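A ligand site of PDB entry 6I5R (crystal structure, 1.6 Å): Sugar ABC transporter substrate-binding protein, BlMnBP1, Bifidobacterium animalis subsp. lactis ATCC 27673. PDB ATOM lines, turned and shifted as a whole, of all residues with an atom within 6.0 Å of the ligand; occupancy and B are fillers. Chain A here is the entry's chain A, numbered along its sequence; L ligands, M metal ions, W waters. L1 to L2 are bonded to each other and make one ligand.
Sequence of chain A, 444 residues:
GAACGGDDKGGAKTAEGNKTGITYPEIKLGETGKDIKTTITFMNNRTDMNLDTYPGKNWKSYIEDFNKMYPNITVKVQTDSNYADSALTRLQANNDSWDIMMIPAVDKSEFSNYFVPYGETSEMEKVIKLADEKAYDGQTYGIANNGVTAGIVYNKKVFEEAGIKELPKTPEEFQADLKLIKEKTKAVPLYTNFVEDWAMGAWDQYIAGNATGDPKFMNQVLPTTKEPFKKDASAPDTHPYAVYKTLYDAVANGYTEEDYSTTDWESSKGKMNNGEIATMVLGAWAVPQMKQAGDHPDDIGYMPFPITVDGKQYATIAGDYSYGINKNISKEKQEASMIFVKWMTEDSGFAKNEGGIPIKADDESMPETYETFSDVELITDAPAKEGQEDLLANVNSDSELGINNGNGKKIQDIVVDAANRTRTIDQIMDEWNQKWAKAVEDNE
O1 of LIG L1 lies within hydrogen-bond range of OE2 of Glu 266, 2.7 Å away.
NZ of Lys 269 sits at hydrogen-bond distance from O2 of LIG L1 (2.9 Å).
The side-chain amide oxygen (OE1) of Gln 289 lies within hydrogen-bond range of an oxygen (O2) of LIG L1, at 2.5 Å.
The backbone carbonyl oxygen (O) of Ser 81 is in hydrogen-bond range of an oxygen (O6) of LIG L1 (3.3 Å).
The indole nitrogen (NE1) of Trp 265 lies within hydrogen-bond range of an oxygen (O2) of LIG L1, at 3.1 Å.
The side-chain amide nitrogen of Asn 45 is in hydrogen-bond range of an oxygen (O1) of LG2 L2 (2.9 Å).
An oxygen (O3) of LG2 L2 sits at hydrogen-bond distance from the side-chain carboxylate (OD1) of Asp 320 (2.7 Å).
The side-chain carboxylate of Glu 196 lies close to the indole nitrogen of Trp 198 (2.9 Å).
OE1 of Gln 289 sits at hydrogen-bond distance from NZ of Lys 269, 3.3 Å away.
O of Tyr 321 lies within hydrogen-bond range of N of Asn 145.
ND2 of Asn 145 sits at hydrogen-bond distance from OD2 of Asp 320, at 3.1 Å.
The side-chain carboxylate (OE1) of Glu 266 is in salt-bridge range of the side-chain amino group (NZ) of Lys 269.
NH2 of Arg 46 lies close to NE2 of Gln 289.
The side-chain carboxylate of Asp 48 lies within salt-bridge range of the guanidinium group of Arg 46.
Merely in contact with the ligand: Arg 46, Thr 47, Asp 48, Trp 198, Trp 285 and Tyr 321.
Hydrophobic or aromatic side chains within 4 Å of the ligand: Trp 198, Trp 265, Trp 285 and Tyr 321.
The nearest printed residue that does not touch the ligand is Glu 196 (4.4 Å).
Water W5 bridges the side-chain hydroxyl (OH) of Tyr 321 (2.6 Å) and an oxygen (O2) of LG2 L2 (2.7 Å).
Water W2 bridges an oxygen (O3) of LG2 L2 (2.8 Å) and the side-chain amide nitrogen (NE2) of Gln 205 (3.5 Å).
Water W1 lies within hydrogen-bond range of O1 of LG2 L2 (2.8 Å) and O of Ser 81 (3.5 Å).
Water W4 bridges an oxygen (O6) of LIG L1 and the backbone carbonyl oxygen (O) of Ser 81.
Water W6 lies within hydrogen-bond range of an oxygen (O5) of LG2 L2 (2.9 Å), the guanidinium group of Arg 46 (3.1 Å) and the side-chain amide nitrogen of Asn 145 (3.5 Å).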
ATOM      1  N   ASN A  45     -18.209   5.416  14.206  1.00  0.00           N
ATOM      2  CA  ASN A  45     -17.439   4.333  14.799  1.00  0.00           C
ATOM      3  C   ASN A  45     -17.872   3.982  16.219  1.00  0.00           C
ATOM      4  O   ASN A  45     -17.329   3.034  16.791  1.00  0.00           O
ATOM      5  CB  ASN A  45     -15.969   4.705  14.841  1.00  0.00           C
ATOM      6  CG  ASN A  45     -15.727   5.958  15.649  1.00  0.00           C
ATOM      7  OD1 ASN A  45     -16.368   6.969  15.451  1.00  0.00           O
ATOM      8  ND2 ASN A  45     -14.802   5.867  16.596  1.00  0.00           N
ATOM      9  N   ARG A  46     -18.779   4.744  16.805  1.00  0.00           N
ATOM     10  CA  ARG A  46     -19.105   4.617  18.219  1.00  0.00           C
ATOM     11  C   ARG A  46     -20.208   3.571  18.390  1.00  0.00           C
ATOM     12  O   ARG A  46     -21.360   3.875  18.707  1.00  0.00           O
ATOM     13  CB  ARG A  46     -19.483   5.971  18.797  1.00  0.00           C
ATOM     14  CG  ARG A  46     -18.316   6.972  18.756  1.00  0.00           C
ATOM     15  CD  ARG A  46     -17.105   6.482  19.601  1.00  0.00           C
ATOM     16  NE  ARG A  46     -17.496   6.176  20.956  1.00  0.00           N
ATOM     17  CZ  ARG A  46     -17.508   7.066  21.943  1.00  0.00           C
ATOM     18  NH1 ARG A  46     -17.145   8.324  21.727  1.00  0.00           N
ATOM     19  NH2 ARG A  46     -17.907   6.692  23.141  1.00  0.00           N
ATOM     20  N   THR A  47     -19.821   2.320  18.169  1.00  0.00           N
ATOM     21  CA  THR A  47     -20.747   1.209  18.401  1.00  0.00           C
ATOM     22  C   THR A  47     -21.282   1.233  19.821  1.00  0.00           C
ATOM     23  O   THR A  47     -22.443   0.889  20.078  1.00  0.00           O
ATOM     24  CB  THR A  47     -20.037  -0.112  18.127  1.00  0.00           C
ATOM     25  OG1 THR A  47     -18.857  -0.187  18.934  1.00  0.00           O
ATOM     26  CG2 THR A  47     -19.636  -0.232  16.696  1.00  0.00           C
ATOM     27  N   ASP A  48     -20.433   1.615  20.777  1.00  0.00           N
ATOM     28  CA  ASP A  48     -20.868   1.682  22.158  1.00  0.00           C
ATOM     29  C   ASP A  48     -22.046   2.645  22.352  1.00  0.00           C
ATOM     30  O   ASP A  48     -22.999   2.324  23.074  1.00  0.00           O
ATOM     31  CB  ASP A  48     -19.676   2.071  23.041  1.00  0.00           C
ATOM     32  CG  ASP A  48     -19.058   3.427  22.674  1.00  0.00           C
ATOM     33  OD1 ASP A  48     -19.197   3.881  21.524  1.00  0.00           O
ATOM     34  OD2 ASP A  48     -18.363   4.001  23.571  1.00  0.00           O
ATOM     35  N   ASP A  80     -20.220   0.476  12.968  1.00  0.00           N
ATOM     36  CA  ASP A  80     -19.455  -0.721  12.617  1.00  0.00           C
ATOM     37  C   ASP A  80     -18.255  -0.874  13.535  1.00  0.00           C
ATOM     38  O   ASP A  80     -17.553   0.098  13.812  1.00  0.00           O
ATOM     39  CB  ASP A  80     -18.959  -0.606  11.181  1.00  0.00           C
ATOM     40  CG  ASP A  80     -19.965  -1.119  10.172  1.00  0.00           C
ATOM     41  OD1 ASP A  80     -20.441  -2.255  10.390  1.00  0.00           O
ATOM     42  OD2 ASP A  80     -20.260  -0.424   9.157  1.00  0.00           O
ATOM     43  N   SER A  81     -17.976  -2.116  13.984  1.00  0.00           N
ATOM     44  CA  SER A  81     -16.819  -2.290  14.853  1.00  0.00           C
ATOM     45  C   SER A  81     -15.535  -2.071  14.078  1.00  0.00           C
ATOM     46  O   SER A  81     -14.582  -1.477  14.595  1.00  0.00           O
ATOM     47  CB  SER A  81     -16.815  -3.667  15.496  1.00  0.00           C
ATOM     48  OG  SER A  81     -16.748  -4.638  14.475  1.00  0.00           O
ATOM     49  N   ASN A  82     -15.488  -2.556  12.844  1.00  0.00           N
ATOM     50  CA  ASN A  82     -14.321  -2.364  11.981  1.00  0.00           C
ATOM     51  C   ASN A  82     -14.490  -1.086  11.167  1.00  0.00           C
ATOM     52  O   ASN A  82     -14.544  -1.084   9.959  1.00  0.00           O
ATOM     53  CB  ASN A  82     -14.129  -3.585  11.083  1.00  0.00           C
ATOM     54  CG  ASN A  82     -12.802  -3.569  10.363  1.00  0.00           C
ATOM     55  OD1 ASN A  82     -11.939  -2.740  10.643  1.00  0.00           O
ATOM     56  ND2 ASN A  82     -12.629  -4.501   9.416  1.00  0.00           N
ATOM     57  N   TYR A  83     -14.580   0.038  11.874  1.00  0.00           N
ATOM     58  CA  TYR A  83     -15.136   1.234  11.252  1.00  0.00           C
ATOM     59  C   TYR A  83     -14.275   1.723  10.086  1.00  0.00           C
ATOM     60  O   TYR A  83     -14.778   1.951   8.982  1.00  0.00           O
ATOM     61  CB  TYR A  83     -15.331   2.372  12.255  1.00  0.00           C
ATOM     62  CG  TYR A  83     -15.866   3.567  11.477  1.00  0.00           C
ATOM     63  CD1 TYR A  83     -17.170   3.578  11.013  1.00  0.00           C
ATOM     64  CD2 TYR A  83     -15.030   4.627  11.106  1.00  0.00           C
ATOM     65  CE1 TYR A  83     -17.659   4.631  10.257  1.00  0.00           C
ATOM     66  CE2 TYR A  83     -15.503   5.687  10.335  1.00  0.00           C
ATOM     67  CZ  TYR A  83     -16.838   5.673   9.929  1.00  0.00           C
ATOM     68  OH  TYR A  83     -17.352   6.710   9.166  1.00  0.00           O
ATOM     69  N   ASN A 145     -15.180  15.970  15.223  1.00  0.00           N
ATOM     70  CA  ASN A 145     -16.223  15.641  16.189  1.00  0.00           C
ATOM     71  C   ASN A 145     -15.907  16.259  17.551  1.00  0.00           C
ATOM     72  O   ASN A 145     -16.811  16.692  18.284  1.00  0.00           O
ATOM     73  CB  ASN A 145     -16.405  14.117  16.284  1.00  0.00           C
ATOM     74  CG  ASN A 145     -15.111  13.356  16.636  1.00  0.00           C
ATOM     75  OD1 ASN A 145     -14.055  13.948  16.773  1.00  0.00           O
ATOM     76  ND2 ASN A 145     -15.223  12.031  16.789  1.00  0.00           N
ATOM     77  N   GLU A 196      -6.712  -4.631  18.097  1.00  0.00           N
ATOM     78  CA  GLU A 196      -7.400  -3.521  17.451  1.00  0.00           C
ATOM     79  C   GLU A 196      -6.403  -2.768  16.569  1.00  0.00           C
ATOM     80  O   GLU A 196      -5.469  -2.119  17.074  1.00  0.00           O
ATOM     81  CB  GLU A 196      -8.023  -2.598  18.482  1.00  0.00           C
ATOM     82  CG  GLU A 196      -9.073  -3.209  19.364  1.00  0.00           C
ATOM     83  CD  GLU A 196     -10.291  -3.728  18.599  1.00  0.00           C
ATOM     84  OE1 GLU A 196     -10.874  -3.001  17.767  1.00  0.00           O
ATOM     85  OE2 GLU A 196     -10.673  -4.871  18.862  1.00  0.00           O
ATOM     86  N   TRP A 198      -6.751  -0.008  15.088  1.00  0.00           N
ATOM     87  CA  TRP A 198      -6.764   1.425  15.332  1.00  0.00           C
ATOM     88  C   TRP A 198      -6.007   1.727  16.623  1.00  0.00           C
ATOM     89  O   TRP A 198      -5.397   2.790  16.737  1.00  0.00           O
ATOM     90  CB  TRP A 198      -8.185   1.968  15.413  1.00  0.00           C
ATOM     91  CG  TRP A 198      -8.986   1.297  16.444  1.00  0.00           C
ATOM     92  CD1 TRP A 198      -9.834   0.249  16.264  1.00  0.00           C
ATOM     93  CD2 TRP A 198      -8.996   1.589  17.847  1.00  0.00           C
ATOM     94  NE1 TRP A 198     -10.381  -0.117  17.476  1.00  0.00           N
ATOM     95  CE2 TRP A 198      -9.856   0.682  18.457  1.00  0.00           C
ATOM     96  CE3 TRP A 198      -8.338   2.528  18.643  1.00  0.00           C
ATOM     97  CZ2 TRP A 198     -10.107   0.694  19.836  1.00  0.00           C
ATOM     98  CZ3 TRP A 198      -8.577   2.539  19.992  1.00  0.00           C
ATOM     99  CH2 TRP A 198      -9.440   1.623  20.574  1.00  0.00           C
ATOM    100  N   GLN A 205       0.125   8.904  16.506  1.00  0.00           N
ATOM    101  CA  GLN A 205      -0.383  10.183  16.939  1.00  0.00           C
ATOM    102  C   GLN A 205       0.592  10.950  17.814  1.00  0.00           C
ATOM    103  O   GLN A 205       0.337  12.112  18.126  1.00  0.00           O
ATOM    104  CB  GLN A 205      -1.686   9.979  17.709  1.00  0.00           C
ATOM    105  CG  GLN A 205      -2.784   9.399  16.830  1.00  0.00           C
ATOM    106  CD  GLN A 205      -4.050   9.054  17.588  1.00  0.00           C
ATOM    107  OE1 GLN A 205      -4.139   9.242  18.801  1.00  0.00           O
ATOM    108  NE2 GLN A 205      -5.044   8.523  16.861  1.00  0.00           N
ATOM    109  N   TRP A 265     -10.375  -5.289  23.545  1.00  0.00           N
ATOM    110  CA  TRP A 265     -10.569  -3.862  23.791  1.00  0.00           C
ATOM    111  C   TRP A 265     -11.632  -3.598  24.839  1.00  0.00           C
ATOM    112  O   TRP A 265     -11.398  -2.846  25.797  1.00  0.00           O
ATOM    113  CB  TRP A 265     -10.926  -3.180  22.467  1.00  0.00           C
ATOM    114  CG  TRP A 265     -11.493  -1.833  22.621  1.00  0.00           C
ATOM    115  CD1 TRP A 265     -12.716  -1.441  22.200  1.00  0.00           C
ATOM    116  CD2 TRP A 265     -10.899  -0.695  23.276  1.00  0.00           C
ATOM    117  NE1 TRP A 265     -12.920  -0.125  22.507  1.00  0.00           N
ATOM    118  CE2 TRP A 265     -11.816   0.356  23.163  1.00  0.00           C
ATOM    119  CE3 TRP A 265      -9.677  -0.470  23.927  1.00  0.00           C
ATOM    120  CZ2 TRP A 265     -11.568   1.643  23.689  1.00  0.00           C
ATOM    121  CZ3 TRP A 265      -9.428   0.827  24.439  1.00  0.00           C
ATOM    122  CH2 TRP A 265     -10.372   1.853  24.319  1.00  0.00           C
ATOM    123  N   GLU A 266     -12.801  -4.219  24.699  1.00  0.00           N
ATOM    124  CA  GLU A 266     -13.938  -3.867  25.547  1.00  0.00           C
ATOM    125  C   GLU A 266     -13.683  -4.247  26.991  1.00  0.00           C
ATOM    126  O   GLU A 266     -14.033  -3.484  27.899  1.00  0.00           O
ATOM    127  CB  GLU A 266     -15.215  -4.542  25.050  1.00  0.00           C
ATOM    128  CG  GLU A 266     -15.732  -3.952  23.758  1.00  0.00           C
ATOM    129  CD  GLU A 266     -16.195  -2.513  23.896  1.00  0.00           C
ATOM    130  OE1 GLU A 266     -16.266  -2.012  25.039  1.00  0.00           O
ATOM    131  OE2 GLU A 266     -16.524  -1.882  22.888  1.00  0.00           O
ATOM    132  N   LYS A 269     -11.238  -1.898  29.087  1.00  0.00           N
ATOM    133  CA  LYS A 269     -11.771  -0.751  29.787  1.00  0.00           C
ATOM    134  C   LYS A 269     -12.012  -1.089  31.255  1.00  0.00           C
ATOM    135  O   LYS A 269     -11.544  -0.380  32.159  1.00  0.00           O
ATOM    136  CB  LYS A 269     -13.093  -0.285  29.132  1.00  0.00           C
ATOM    137  CG  LYS A 269     -12.933   0.331  27.739  1.00  0.00           C
ATOM    138  CD  LYS A 269     -14.290   0.488  27.112  1.00  0.00           C
ATOM    139  CE  LYS A 269     -14.180   0.759  25.606  1.00  0.00           C
ATOM    140  NZ  LYS A 269     -15.543   0.846  24.970  1.00  0.00           N
ATOM    141  N   TRP A 285     -10.000  10.953  24.386  1.00  0.00           N
ATOM    142  CA  TRP A 285     -11.353  10.428  24.243  1.00  0.00           C
ATOM    143  C   TRP A 285     -11.572   9.162  25.061  1.00  0.00           C
ATOM    144  O   TRP A 285     -12.719   8.834  25.382  1.00  0.00           O
ATOM    145  CB  TRP A 285     -11.647  10.155  22.755  1.00  0.00           C
ATOM    146  CG  TRP A 285     -10.646   9.232  22.195  1.00  0.00           C
ATOM    147  CD1 TRP A 285      -9.524   9.561  21.515  1.00  0.00           C
ATOM    148  CD2 TRP A 285     -10.667   7.799  22.271  1.00  0.00           C
ATOM    149  NE1 TRP A 285      -8.833   8.429  21.169  1.00  0.00           N
ATOM    150  CE2 TRP A 285      -9.512   7.338  21.631  1.00  0.00           C
ATOM    151  CE3 TRP A 285     -11.540   6.876  22.831  1.00  0.00           C
ATOM    152  CZ2 TRP A 285      -9.200   5.998  21.531  1.00  0.00           C
ATOM    153  CZ3 TRP A 285     -11.236   5.537  22.738  1.00  0.00           C
ATOM    154  CH2 TRP A 285     -10.090   5.108  22.072  1.00  0.00           C
ATOM    155  N   GLN A 289     -14.448   6.727  28.782  1.00  0.00           N
ATOM    156  CA  GLN A 289     -14.810   5.324  28.563  1.00  0.00           C
ATOM    157  C   GLN A 289     -14.193   4.414  29.614  1.00  0.00           C
ATOM    158  O   GLN A 289     -14.789   3.400  30.004  1.00  0.00           O
ATOM    159  CB  GLN A 289     -14.378   4.901  27.165  1.00  0.00           C
ATOM    160  CG  GLN A 289     -15.081   5.604  26.041  1.00  0.00           C
ATOM    161  CD  GLN A 289     -14.745   5.047  24.672  1.00  0.00           C
ATOM    162  OE1 GLN A 289     -14.426   3.879  24.512  1.00  0.00           O
ATOM    163  NE2 GLN A 289     -14.808   5.901  23.678  1.00  0.00           N
ATOM    164  N   ASP A 320     -10.397  14.005  16.386  1.00  0.00           N
ATOM    165  CA  ASP A 320     -10.458  12.549  16.470  1.00  0.00           C
ATOM    166  C   ASP A 320     -10.970  11.947  15.160  1.00  0.00           C
ATOM    167  O   ASP A 320     -10.251  11.213  14.470  1.00  0.00           O
ATOM    168  CB  ASP A 320     -11.341  12.135  17.646  1.00  0.00           C
ATOM    169  CG  ASP A 320     -11.640  10.664  17.642  1.00  0.00           C
ATOM    170  OD1 ASP A 320     -10.715   9.835  17.782  1.00  0.00           O
ATOM    171  OD2 ASP A 320     -12.806  10.317  17.530  1.00  0.00           O
ATOM    172  N   TYR A 321     -12.189  12.317  14.773  1.00  0.00           N
ATOM    173  CA  TYR A 321     -12.844  11.884  13.552  1.00  0.00           C
ATOM    174  C   TYR A 321     -13.710  13.044  13.064  1.00  0.00           C
ATOM    175  O   TYR A 321     -14.390  13.688  13.871  1.00  0.00           O
ATOM    176  CB  TYR A 321     -13.719  10.661  13.779  1.00  0.00           C
ATOM    177  CG  TYR A 321     -13.140   9.349  13.306  1.00  0.00           C
ATOM    178  CD1 TYR A 321     -12.864   9.117  11.970  1.00  0.00           C
ATOM    179  CD2 TYR A 321     -12.922   8.314  14.196  1.00  0.00           C
ATOM    180  CE1 TYR A 321     -12.385   7.915  11.526  1.00  0.00           C
ATOM    181  CE2 TYR A 321     -12.422   7.107  13.772  1.00  0.00           C
ATOM    182  CZ  TYR A 321     -12.170   6.901  12.423  1.00  0.00           C
ATOM    183  OH  TYR A 321     -11.675   5.675  11.985  1.00  0.00           O
HETATM  184  C1  LIG L   1     -16.278   1.252  20.936  1.00  0.00           C
HETATM  185  C2  LIG L   1     -15.772   2.602  21.495  1.00  0.00           C
HETATM  186  C3  LIG L   1     -14.997   3.340  20.402  1.00  0.00           C
HETATM  187  C4  LIG L   1     -14.040   2.419  19.696  1.00  0.00           C
HETATM  188  C5  LIG L   1     -14.739   1.124  19.254  1.00  0.00           C
HETATM  189  C6  LIG L   1     -13.800   0.196  18.506  1.00  0.00           C
HETATM  190  O1  LIG L   1     -16.816   0.621  22.049  1.00  0.00           O
HETATM  191  O2  LIG L   1     -14.815   2.309  22.554  1.00  0.00           O
HETATM  192  O3  LIG L   1     -14.312   4.433  20.903  1.00  0.00           O
HETATM  193  O4  LIG L   1     -13.496   3.060  18.534  1.00  0.00           O
HETATM  194  O5  LIG L   1     -15.277   0.482  20.395  1.00  0.00           O
HETATM  195  O6  LIG L   1     -14.644  -0.731  17.812  1.00  0.00           O
HETATM  196  C1  LG2 L   2     -12.469   3.992  18.689  1.00  0.00           C
HETATM  197  C2  LG2 L   2     -11.683   3.868  17.346  1.00  0.00           C
HETATM  198  C3  LG2 L   2     -10.634   4.932  17.313  1.00  0.00           C
HETATM  199  C4  LG2 L   2     -11.199   6.294  17.708  1.00  0.00           C
HETATM  200  C5  LG2 L   2     -11.915   6.222  19.064  1.00  0.00           C
HETATM  201  C6  LG2 L   2     -12.554   7.547  19.426  1.00  0.00           C
HETATM  202  O1  LG2 L   2     -12.524   4.180  16.239  1.00  0.00           O
HETATM  203  O2  LG2 L   2     -10.000   5.049  16.040  1.00  0.00           O
HETATM  204  O3  LG2 L   2     -10.130   7.199  17.811  1.00  0.00           O
HETATM  205  O4  LG2 L   2     -12.953   5.250  18.958  1.00  0.00           O
HETATM  206  O5  LG2 L   2     -13.597   7.884  18.499  1.00  0.00           O
HETATM  207 ZN    ZN M   1     -12.159  -3.756  16.128  1.00  0.00          ZN
HETATM  208  O   HOH W   1     -13.214   1.620  15.281  1.00  0.00           O
HETATM  209  O   HOH W   2      -7.480   6.544  18.372  1.00  0.00           O
HETATM  210  O   HOH W   3     -15.761   1.008  15.623  1.00  0.00           O
HETATM  211  O   HOH W   4     -13.611  -3.135  16.722  1.00  0.00           O
HETATM  212  O   HOH W   5     -10.524   3.931  13.584  1.00  0.00           O
HETATM  213  O   HOH W   6     -15.834   9.588  19.187  1.00  0.00           O
